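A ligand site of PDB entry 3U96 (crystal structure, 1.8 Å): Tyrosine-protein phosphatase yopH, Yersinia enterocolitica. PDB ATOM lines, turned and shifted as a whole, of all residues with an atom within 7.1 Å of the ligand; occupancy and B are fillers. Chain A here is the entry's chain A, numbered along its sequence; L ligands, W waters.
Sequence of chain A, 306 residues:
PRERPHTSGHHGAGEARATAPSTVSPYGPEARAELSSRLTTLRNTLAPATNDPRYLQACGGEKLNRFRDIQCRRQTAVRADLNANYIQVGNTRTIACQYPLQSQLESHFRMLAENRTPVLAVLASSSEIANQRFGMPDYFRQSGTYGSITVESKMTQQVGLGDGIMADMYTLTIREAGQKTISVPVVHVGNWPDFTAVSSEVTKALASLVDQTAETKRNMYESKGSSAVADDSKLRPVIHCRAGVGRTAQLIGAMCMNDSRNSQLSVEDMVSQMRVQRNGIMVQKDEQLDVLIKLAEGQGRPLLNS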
ATOM      1  N   ARG A  66      39.302  -6.824  21.787  1.00  0.00           N
ATOM      2  CA  ARG A  66      38.835  -7.474  23.014  1.00  0.00           C
ATOM      3  C   ARG A  66      38.221  -8.846  22.711  1.00  0.00           C
ATOM      4  O   ARG A  66      38.388  -9.811  23.485  1.00  0.00           O
ATOM      5  CB  ARG A  66      37.849  -6.567  23.752  1.00  0.00           C
ATOM      6  CG  ARG A  66      37.204  -7.189  24.991  1.00  0.00           C
ATOM      7  CD  ARG A  66      36.359  -6.189  25.725  1.00  0.00           C
ATOM      8  NE  ARG A  66      37.154  -5.133  26.366  1.00  0.00           N
ATOM      9  CZ  ARG A  66      37.790  -5.274  27.530  1.00  0.00           C
ATOM     10  NH1 ARG A  66      38.469  -4.244  28.042  1.00  0.00           N
ATOM     11  NH2 ARG A  66      37.792  -6.442  28.180  1.00  0.00           N
ATOM     12  N   PHE A  67      37.513  -8.931  21.572  1.00  0.00           N
ATOM     13  CA  PHE A  67      36.959 -10.185  21.067  1.00  0.00           C
ATOM     14  C   PHE A  67      37.473 -10.417  19.659  1.00  0.00           C
ATOM     15  O   PHE A  67      37.476  -9.530  18.833  1.00  0.00           O
ATOM     16  CB  PHE A  67      35.417 -10.199  21.075  1.00  0.00           C
ATOM     17  CG  PHE A  67      34.842  -9.950  22.440  1.00  0.00           C
ATOM     18  CD1 PHE A  67      34.764 -10.987  23.367  1.00  0.00           C
ATOM     19  CD2 PHE A  67      34.460  -8.666  22.821  1.00  0.00           C
ATOM     20  CE1 PHE A  67      34.278 -10.755  24.664  1.00  0.00           C
ATOM     21  CE2 PHE A  67      33.963  -8.416  24.111  1.00  0.00           C
ATOM     22  CZ  PHE A  67      33.868  -9.465  25.032  1.00  0.00           C
ATOM     23  N   ARG A  68      37.874 -11.656  19.391  1.00  0.00           N
ATOM     24  CA  ARG A  68      38.532 -11.997  18.148  1.00  0.00           C
ATOM     25  C   ARG A  68      37.725 -11.587  16.915  1.00  0.00           C
ATOM     26  O   ARG A  68      38.263 -11.085  15.936  1.00  0.00           O
ATOM     27  CB  ARG A  68      38.789 -13.517  18.115  1.00  0.00           C
ATOM     28  CG  ARG A  68      39.445 -14.018  16.840  1.00  0.00           C
ATOM     29  CD  ARG A  68      39.615 -15.537  16.901  1.00  0.00           C
ATOM     30  NE  ARG A  68      38.311 -16.181  17.092  1.00  0.00           N
ATOM     31  CZ  ARG A  68      38.098 -17.481  17.281  1.00  0.00           C
ATOM     32  NH1 ARG A  68      36.859 -17.919  17.447  1.00  0.00           N
ATOM     33  NH2 ARG A  68      39.120 -18.331  17.311  1.00  0.00           N
ATOM     34  N   ASP A  69      36.422 -11.818  17.017  1.00  0.00           N
ATOM     35  CA  ASP A  69      35.474 -11.720  15.924  1.00  0.00           C
ATOM     36  C   ASP A  69      34.810 -10.336  15.853  1.00  0.00           C
ATOM     37  O   ASP A  69      33.930 -10.120  15.009  1.00  0.00           O
ATOM     38  CB  ASP A  69      34.372 -12.752  16.185  1.00  0.00           C
ATOM     39  CG  ASP A  69      33.946 -12.792  17.679  1.00  0.00           C
ATOM     40  OD1 ASP A  69      34.826 -12.975  18.585  1.00  0.00           O
ATOM     41  OD2 ASP A  69      32.730 -12.651  17.963  1.00  0.00           O
ATOM     42  N   ILE A  70      35.195  -9.426  16.749  1.00  0.00           N
ATOM     43  CA  ILE A  70      34.588  -8.086  16.791  1.00  0.00           C
ATOM     44  C   ILE A  70      35.655  -7.070  16.415  1.00  0.00           C
ATOM     45  O   ILE A  70      36.473  -6.634  17.269  1.00  0.00           O
ATOM     46  CB  ILE A  70      33.988  -7.733  18.172  1.00  0.00           C
ATOM     47  CG1 ILE A  70      32.930  -8.738  18.650  1.00  0.00           C
ATOM     48  CG2 ILE A  70      33.374  -6.324  18.154  1.00  0.00           C
ATOM     49  CD1 ILE A  70      31.684  -8.892  17.749  1.00  0.00           C
ATOM     50  N   LEU A 123      28.213   1.922  28.994  1.00  0.00           N
ATOM     51  CA  LEU A 123      27.026   1.091  29.171  1.00  0.00           C
ATOM     52  C   LEU A 123      27.354  -0.281  29.740  1.00  0.00           C
ATOM     53  O   LEU A 123      26.448  -1.073  29.943  1.00  0.00           O
ATOM     54  CB  LEU A 123      26.282   0.901  27.831  1.00  0.00           C
ATOM     55  CG  LEU A 123      26.094   2.201  27.049  1.00  0.00           C
ATOM     56  CD1 LEU A 123      25.389   1.940  25.750  1.00  0.00           C
ATOM     57  CD2 LEU A 123      25.349   3.236  27.869  1.00  0.00           C
ATOM     58  N   ALA A 124      28.633  -0.550  30.011  1.00  0.00           N
ATOM     59  CA  ALA A 124      29.018  -1.730  30.800  1.00  0.00           C
ATOM     60  C   ALA A 124      28.635  -1.477  32.255  1.00  0.00           C
ATOM     61  O   ALA A 124      28.787  -0.371  32.751  1.00  0.00           O
ATOM     62  CB  ALA A 124      30.496  -1.986  30.693  1.00  0.00           C
ATOM     63  N   GLU A 128      30.029  -5.946  35.693  1.00  0.00           N
ATOM     64  CA  GLU A 128      30.999  -6.321  34.659  1.00  0.00           C
ATOM     65  C   GLU A 128      32.386  -5.746  34.955  1.00  0.00           C
ATOM     66  O   GLU A 128      33.372  -6.456  34.834  1.00  0.00           O
ATOM     67  CB  GLU A 128      30.567  -5.852  33.259  1.00  0.00           C
ATOM     68  CG  GLU A 128      29.387  -6.546  32.644  1.00  0.00           C
ATOM     69  CD  GLU A 128      28.900  -5.808  31.386  1.00  0.00           C
ATOM     70  OE1 GLU A 128      28.017  -4.921  31.528  1.00  0.00           O
ATOM     71  OE2 GLU A 128      29.415  -6.079  30.288  1.00  0.00           O
ATOM     72  N   MET A 136      38.167  -5.355  32.331  1.00  0.00           N
ATOM     73  CA  MET A 136      37.579  -4.025  32.014  1.00  0.00           C
ATOM     74  C   MET A 136      37.985  -3.047  33.133  1.00  0.00           C
ATOM     75  O   MET A 136      37.348  -3.031  34.182  1.00  0.00           O
ATOM     76  CB  MET A 136      36.044  -4.112  31.860  1.00  0.00           C
ATOM     77  CG  MET A 136      35.590  -5.025  30.674  1.00  0.00           C
ATOM     78  SD  MET A 136      33.916  -5.700  30.862  1.00  0.00           S
ATOM     79  CE  MET A 136      32.937  -4.262  30.432  1.00  0.00           C
ATOM     80  N   TRP A 192      23.101  -1.483  34.150  1.00  0.00           N
ATOM     81  CA  TRP A 192      22.579  -2.111  32.931  1.00  0.00           C
ATOM     82  C   TRP A 192      22.502  -3.611  33.240  1.00  0.00           C
ATOM     83  O   TRP A 192      23.485  -4.208  33.680  1.00  0.00           O
ATOM     84  CB  TRP A 192      23.475  -1.843  31.712  1.00  0.00           C
ATOM     85  CG  TRP A 192      22.799  -2.204  30.410  1.00  0.00           C
ATOM     86  CD1 TRP A 192      22.429  -3.462  30.015  1.00  0.00           C
ATOM     87  CD2 TRP A 192      22.444  -1.323  29.348  1.00  0.00           C
ATOM     88  NE1 TRP A 192      21.827  -3.394  28.778  1.00  0.00           N
ATOM     89  CE2 TRP A 192      21.816  -2.100  28.349  1.00  0.00           C
ATOM     90  CE3 TRP A 192      22.543   0.059  29.159  1.00  0.00           C
ATOM     91  CZ2 TRP A 192      21.335  -1.544  27.147  1.00  0.00           C
ATOM     92  CZ3 TRP A 192      22.067   0.618  27.969  1.00  0.00           C
ATOM     93  CH2 TRP A 192      21.469  -0.183  26.988  1.00  0.00           C
ATOM     94  N   HIS A 240      30.699   3.453  24.565  1.00  0.00           N
ATOM     95  CA  HIS A 240      31.072   2.039  24.604  1.00  0.00           C
ATOM     96  C   HIS A 240      30.316   1.244  25.639  1.00  0.00           C
ATOM     97  O   HIS A 240      29.871   1.780  26.650  1.00  0.00           O
ATOM     98  CB  HIS A 240      32.583   1.822  24.730  1.00  0.00           C
ATOM     99  CG  HIS A 240      33.170   2.133  26.076  1.00  0.00           C
ATOM    100  ND1 HIS A 240      33.089   1.268  27.141  1.00  0.00           N
ATOM    101  CD2 HIS A 240      33.953   3.161  26.481  1.00  0.00           C
ATOM    102  CE1 HIS A 240      33.747   1.788  28.174  1.00  0.00           C
ATOM    103  NE2 HIS A 240      34.274   2.931  27.790  1.00  0.00           N
ATOM    104  N   CYS A 241      30.142  -0.045  25.364  1.00  0.00           N
ATOM    105  CA  CYS A 241      29.650  -0.994  26.337  1.00  0.00           C
ATOM    106  C   CYS A 241      30.829  -1.953  26.628  1.00  0.00           C
ATOM    107  O   CYS A 241      31.886  -1.500  27.066  1.00  0.00           O
ATOM    108  CB  CYS A 241      28.410  -1.738  25.803  1.00  0.00           C
ATOM    109  SG  CYS A 241      28.488  -2.225  24.028  1.00  0.00           S
ATOM    110  N   ARG A 242      30.674  -3.248  26.362  1.00  0.00           N
ATOM    111  CA  ARG A 242      31.812  -4.173  26.483  1.00  0.00           C
ATOM    112  C   ARG A 242      32.497  -4.390  25.131  1.00  0.00           C
ATOM    113  O   ARG A 242      33.667  -4.069  24.918  1.00  0.00           O
ATOM    114  CB  ARG A 242      31.386  -5.499  27.134  1.00  0.00           C
ATOM    115  CG  ARG A 242      32.541  -6.459  27.481  1.00  0.00           C
ATOM    116  CD  ARG A 242      32.061  -7.611  28.358  1.00  0.00           C
ATOM    117  NE  ARG A 242      33.057  -8.675  28.355  1.00  0.00           N
ATOM    118  CZ  ARG A 242      32.799  -9.946  28.608  1.00  0.00           C
ATOM    119  NH1 ARG A 242      31.560 -10.347  28.858  1.00  0.00           N
ATOM    120  NH2 ARG A 242      33.775 -10.837  28.557  1.00  0.00           N
ATOM    121  N   ALA A 243      31.730  -4.905  24.169  1.00  0.00           N
ATOM    122  CA  ALA A 243      32.263  -5.073  22.816  1.00  0.00           C
ATOM    123  C   ALA A 243      32.055  -3.846  21.935  1.00  0.00           C
ATOM    124  O   ALA A 243      32.693  -3.744  20.912  1.00  0.00           O
ATOM    125  CB  ALA A 243      31.682  -6.351  22.155  1.00  0.00           C
ATOM    126  N   GLY A 244      31.158  -2.941  22.324  1.00  0.00           N
ATOM    127  CA  GLY A 244      30.831  -1.791  21.467  1.00  0.00           C
ATOM    128  C   GLY A 244      29.988  -2.150  20.241  1.00  0.00           C
ATOM    129  O   GLY A 244      30.083  -1.460  19.212  1.00  0.00           O
ATOM    130  N   VAL A 245      29.159  -3.196  20.320  1.00  0.00           N
ATOM    131  CA  VAL A 245      28.300  -3.603  19.174  1.00  0.00           C
ATOM    132  C   VAL A 245      26.817  -3.819  19.524  1.00  0.00           C
ATOM    133  O   VAL A 245      25.933  -3.820  18.623  1.00  0.00           O
ATOM    134  CB  VAL A 245      28.802  -4.895  18.403  1.00  0.00           C
ATOM    135  CG1 VAL A 245      30.129  -4.632  17.737  1.00  0.00           C
ATOM    136  CG2 VAL A 245      28.825  -6.147  19.334  1.00  0.00           C
ATOM    137  N   GLY A 246      26.534  -4.089  20.787  1.00  0.00           N
ATOM    138  CA  GLY A 246      25.166  -4.426  21.200  1.00  0.00           C
ATOM    139  C   GLY A 246      24.505  -3.221  21.864  1.00  0.00           C
ATOM    140  O   GLY A 246      23.733  -2.479  21.243  1.00  0.00           O
ATOM    141  N   ARG A 247      24.811  -3.028  23.141  1.00  0.00           N
ATOM    142  CA  ARG A 247      24.232  -1.923  23.884  1.00  0.00           C
ATOM    143  C   ARG A 247      24.586  -0.562  23.281  1.00  0.00           C
ATOM    144  O   ARG A 247      23.736   0.366  23.208  1.00  0.00           O
ATOM    145  CB  ARG A 247      24.662  -2.031  25.347  1.00  0.00           C
ATOM    146  CG  ARG A 247      24.101  -3.296  26.004  1.00  0.00           C
ATOM    147  CD  ARG A 247      24.752  -3.518  27.366  1.00  0.00           C
ATOM    148  NE  ARG A 247      26.068  -4.154  27.222  1.00  0.00           N
ATOM    149  CZ  ARG A 247      26.855  -4.452  28.259  1.00  0.00           C
ATOM    150  NH1 ARG A 247      26.452  -4.111  29.501  1.00  0.00           N
ATOM    151  NH2 ARG A 247      28.024  -5.060  28.063  1.00  0.00           N
ATOM    152  N   THR A 248      25.839  -0.469  22.821  1.00  0.00           N
ATOM    153  CA  THR A 248      26.314   0.732  22.134  1.00  0.00           C
ATOM    154  C   THR A 248      25.468   1.055  20.897  1.00  0.00           C
ATOM    155  O   THR A 248      25.078   2.206  20.725  1.00  0.00           O
ATOM    156  CB  THR A 248      27.810   0.579  21.773  1.00  0.00           C
ATOM    157  OG1 THR A 248      28.573   0.630  22.976  1.00  0.00           O
ATOM    158  CG2 THR A 248      28.279   1.650  20.802  1.00  0.00           C
ATOM    159  N   ALA A 249      25.178   0.065  20.070  1.00  0.00           N
ATOM    160  CA  ALA A 249      24.410   0.304  18.839  1.00  0.00           C
ATOM    161  C   ALA A 249      22.967   0.672  19.123  1.00  0.00           C
ATOM    162  O   ALA A 249      22.351   1.505  18.438  1.00  0.00           O
ATOM    163  CB  ALA A 249      24.509  -0.893  17.940  1.00  0.00           C
ATOM    164  N   ILE A 281      28.468  -6.718  13.127  1.00  0.00           N
ATOM    165  CA  ILE A 281      27.730  -7.132  14.321  1.00  0.00           C
ATOM    166  C   ILE A 281      26.917  -6.005  14.960  1.00  0.00           C
ATOM    167  O   ILE A 281      26.050  -6.278  15.790  1.00  0.00           O
ATOM    168  CB  ILE A 281      28.676  -7.812  15.373  1.00  0.00           C
ATOM    169  CG1 ILE A 281      29.554  -8.871  14.687  1.00  0.00           C
ATOM    170  CG2 ILE A 281      27.841  -8.447  16.523  1.00  0.00           C
ATOM    171  CD1 ILE A 281      28.730 -10.011  14.046  1.00  0.00           C
ATOM    172  N   GLN A 284      23.621  -6.263  17.824  1.00  0.00           N
ATOM    173  CA  GLN A 284      24.011  -7.665  17.868  1.00  0.00           C
ATOM    174  C   GLN A 284      22.831  -8.622  18.079  1.00  0.00           C
ATOM    175  O   GLN A 284      22.825  -9.736  17.531  1.00  0.00           O
ATOM    176  CB  GLN A 284      25.036  -7.866  18.980  1.00  0.00           C
ATOM    177  CG  GLN A 284      25.541  -9.313  19.109  1.00  0.00           C
ATOM    178  CD  GLN A 284      26.631  -9.423  20.136  1.00  0.00           C
ATOM    179  OE1 GLN A 284      27.720  -9.960  19.868  1.00  0.00           O
ATOM    180  NE2 GLN A 284      26.367  -8.870  21.308  1.00  0.00           N
ATOM    181  N   LYS A 285      21.854  -8.192  18.833  1.00  0.00           N
ATOM    182  CA  LYS A 285      20.793  -9.063  19.265  1.00  0.00           C
ATOM    183  C   LYS A 285      19.453  -8.673  18.711  1.00  0.00           C
ATOM    184  O   LYS A 285      19.236  -7.535  18.456  1.00  0.00           O
ATOM    185  CB  LYS A 285      20.708  -9.100  20.786  1.00  0.00           C
ATOM    186  CG  LYS A 285      22.000  -9.374  21.377  1.00  0.00           C
ATOM    187  CD  LYS A 285      21.947 -10.297  22.453  1.00  0.00           C
ATOM    188  CE  LYS A 285      21.832  -9.536  23.729  1.00  0.00           C
ATOM    189  NZ  LYS A 285      21.490 -10.329  25.005  1.00  0.00           N
ATOM    190  N   GLN A 288      17.667  -5.888  20.610  1.00  0.00           N
ATOM    191  CA  GLN A 288      18.235  -4.565  20.339  1.00  0.00           C
ATOM    192  C   GLN A 288      17.609  -3.949  19.091  1.00  0.00           C
ATOM    193  O   GLN A 288      17.206  -2.775  19.089  1.00  0.00           O
ATOM    194  CB  GLN A 288      19.755  -4.680  20.206  1.00  0.00           C
ATOM    195  CG  GLN A 288      20.415  -4.972  21.574  1.00  0.00           C
ATOM    196  CD  GLN A 288      21.791  -5.591  21.489  1.00  0.00           C
ATOM    197  OE1 GLN A 288      22.341  -5.837  20.402  1.00  0.00           O
ATOM    198  NE2 GLN A 288      22.374  -5.846  22.668  1.00  0.00           N
HETATM  199  S1  LIG L   1      27.878  -5.655  24.074  1.00  0.00           S
HETATM  200  O1  LIG L   1      27.493  -7.145  24.202  1.00  0.00           O
HETATM  201  O2  LIG L   1      28.365  -5.324  22.730  1.00  0.00           O
HETATM  202  O3  LIG L   1      26.612  -4.999  24.396  1.00  0.00           O
HETATM  203  O4  LIG L   1      28.925  -5.371  25.095  1.00  0.00           O
HETATM  204  O5  LIG L   1      28.166  -8.010  26.631  1.00  0.00           O
HETATM  205  O6  LIG L   1      30.082 -10.161  21.089  1.00  0.00           O
HETATM  206  O7  LIG L   1      31.913 -10.023  22.125  1.00  0.00           O
HETATM  207  C1  LIG L   1      29.089  -8.516  23.146  1.00  0.00           C
HETATM  208  N1  LIG L   1      30.705  -9.913  22.105  1.00  0.00           N
HETATM  209  C2  LIG L   1      29.858  -9.452  25.689  1.00  0.00           C
HETATM  210  C3  LIG L   1      28.477  -8.069  24.293  1.00  0.00           C
HETATM  211  C4  LIG L   1      30.480  -9.932  24.530  1.00  0.00           C
HETATM  212  C5  LIG L   1      28.852  -8.507  25.561  1.00  0.00           C
HETATM  213  C6  LIG L   1      30.086  -9.472  23.272  1.00  0.00           C
HETATM  214  O   HOH W   1      24.750  -7.503  22.958  1.00  0.00           O
HETATM  215  O   HOH W   2      29.216  -8.637  29.369  1.00  0.00           O
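An oxygen (O6) of the ligand sits close to the side-chain amide oxygen (OE1) of Gln 284 (2.7 Å). The backbone NH (N) of Gly 246 sits at hydrogen-bond distance from an oxygen (O2) of the ligand, at 2.9 Å. The backbone NH (N) of Arg 247 lies within hydrogen-bond range of an oxygen (O3) of the ligand. An oxygen (O3) of the ligand is in salt-bridge range of the guanidinium group (NE) of Arg 247. The backbone NH (N) of Ala 243 lies within hydrogen-bond range of an oxygen (O4) of the ligand (3.0 Å). An oxygen (O4) of the ligand is in hydrogen-bond range of the backbone NH (N) of Arg 242 (3.0 Å). The backbone NH (N) of Val 245 is in hydrogen-bond range of an oxygen (O2) of the ligand. The side-chain sulfur of Cys 241 sits at hydrogen-bond distance from an oxygen (O4) of the ligand (3.4 Å).
Water W2 lies within hydrogen-bond range of OE2 of Glu 128, NH1 of Arg 242 and O5 of the ligand. Water W1 lies within hydrogen-bond range of NE2 of Gln 284, NE2 of Gln 288 and O1 of the ligand.
Phe 67 touches the ligand. Ile 70 touches the ligand (CG1 to O7, 3.8 Å). Gly 244 touches the ligand (N to O2, 3.7 Å). Hydrophobic or aromatic side chains within 4 Å of the ligand: Phe 67, Ile 70, Ala 243 and Val 245. The nearest printed residue that does not touch the ligand is Glu 128 (4.3 Å).
The backbone NH of Gln 284 is in hydrogen-bond range of the backbone carbonyl oxygen of Val 245 (3.5 Å). OE1 of Gln 288 is in hydrogen-bond range of N of Gln 284 (2.9 Å). NH1 of Arg 247 lies within salt-bridge range of OE1 of Glu 128 (2.7 Å). NH1 of Arg 247 sits at hydrogen-bond distance from O of Leu 123 (3.1 Å). The backbone NH (N) of Gly 244 sits at hydrogen-bond distance from the side-chain sulfur (SG) of Cys 241 (3.2 Å). N of Cys 241 lies within hydrogen-bond range of OG1 of Thr 248, 2.9 Å away.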
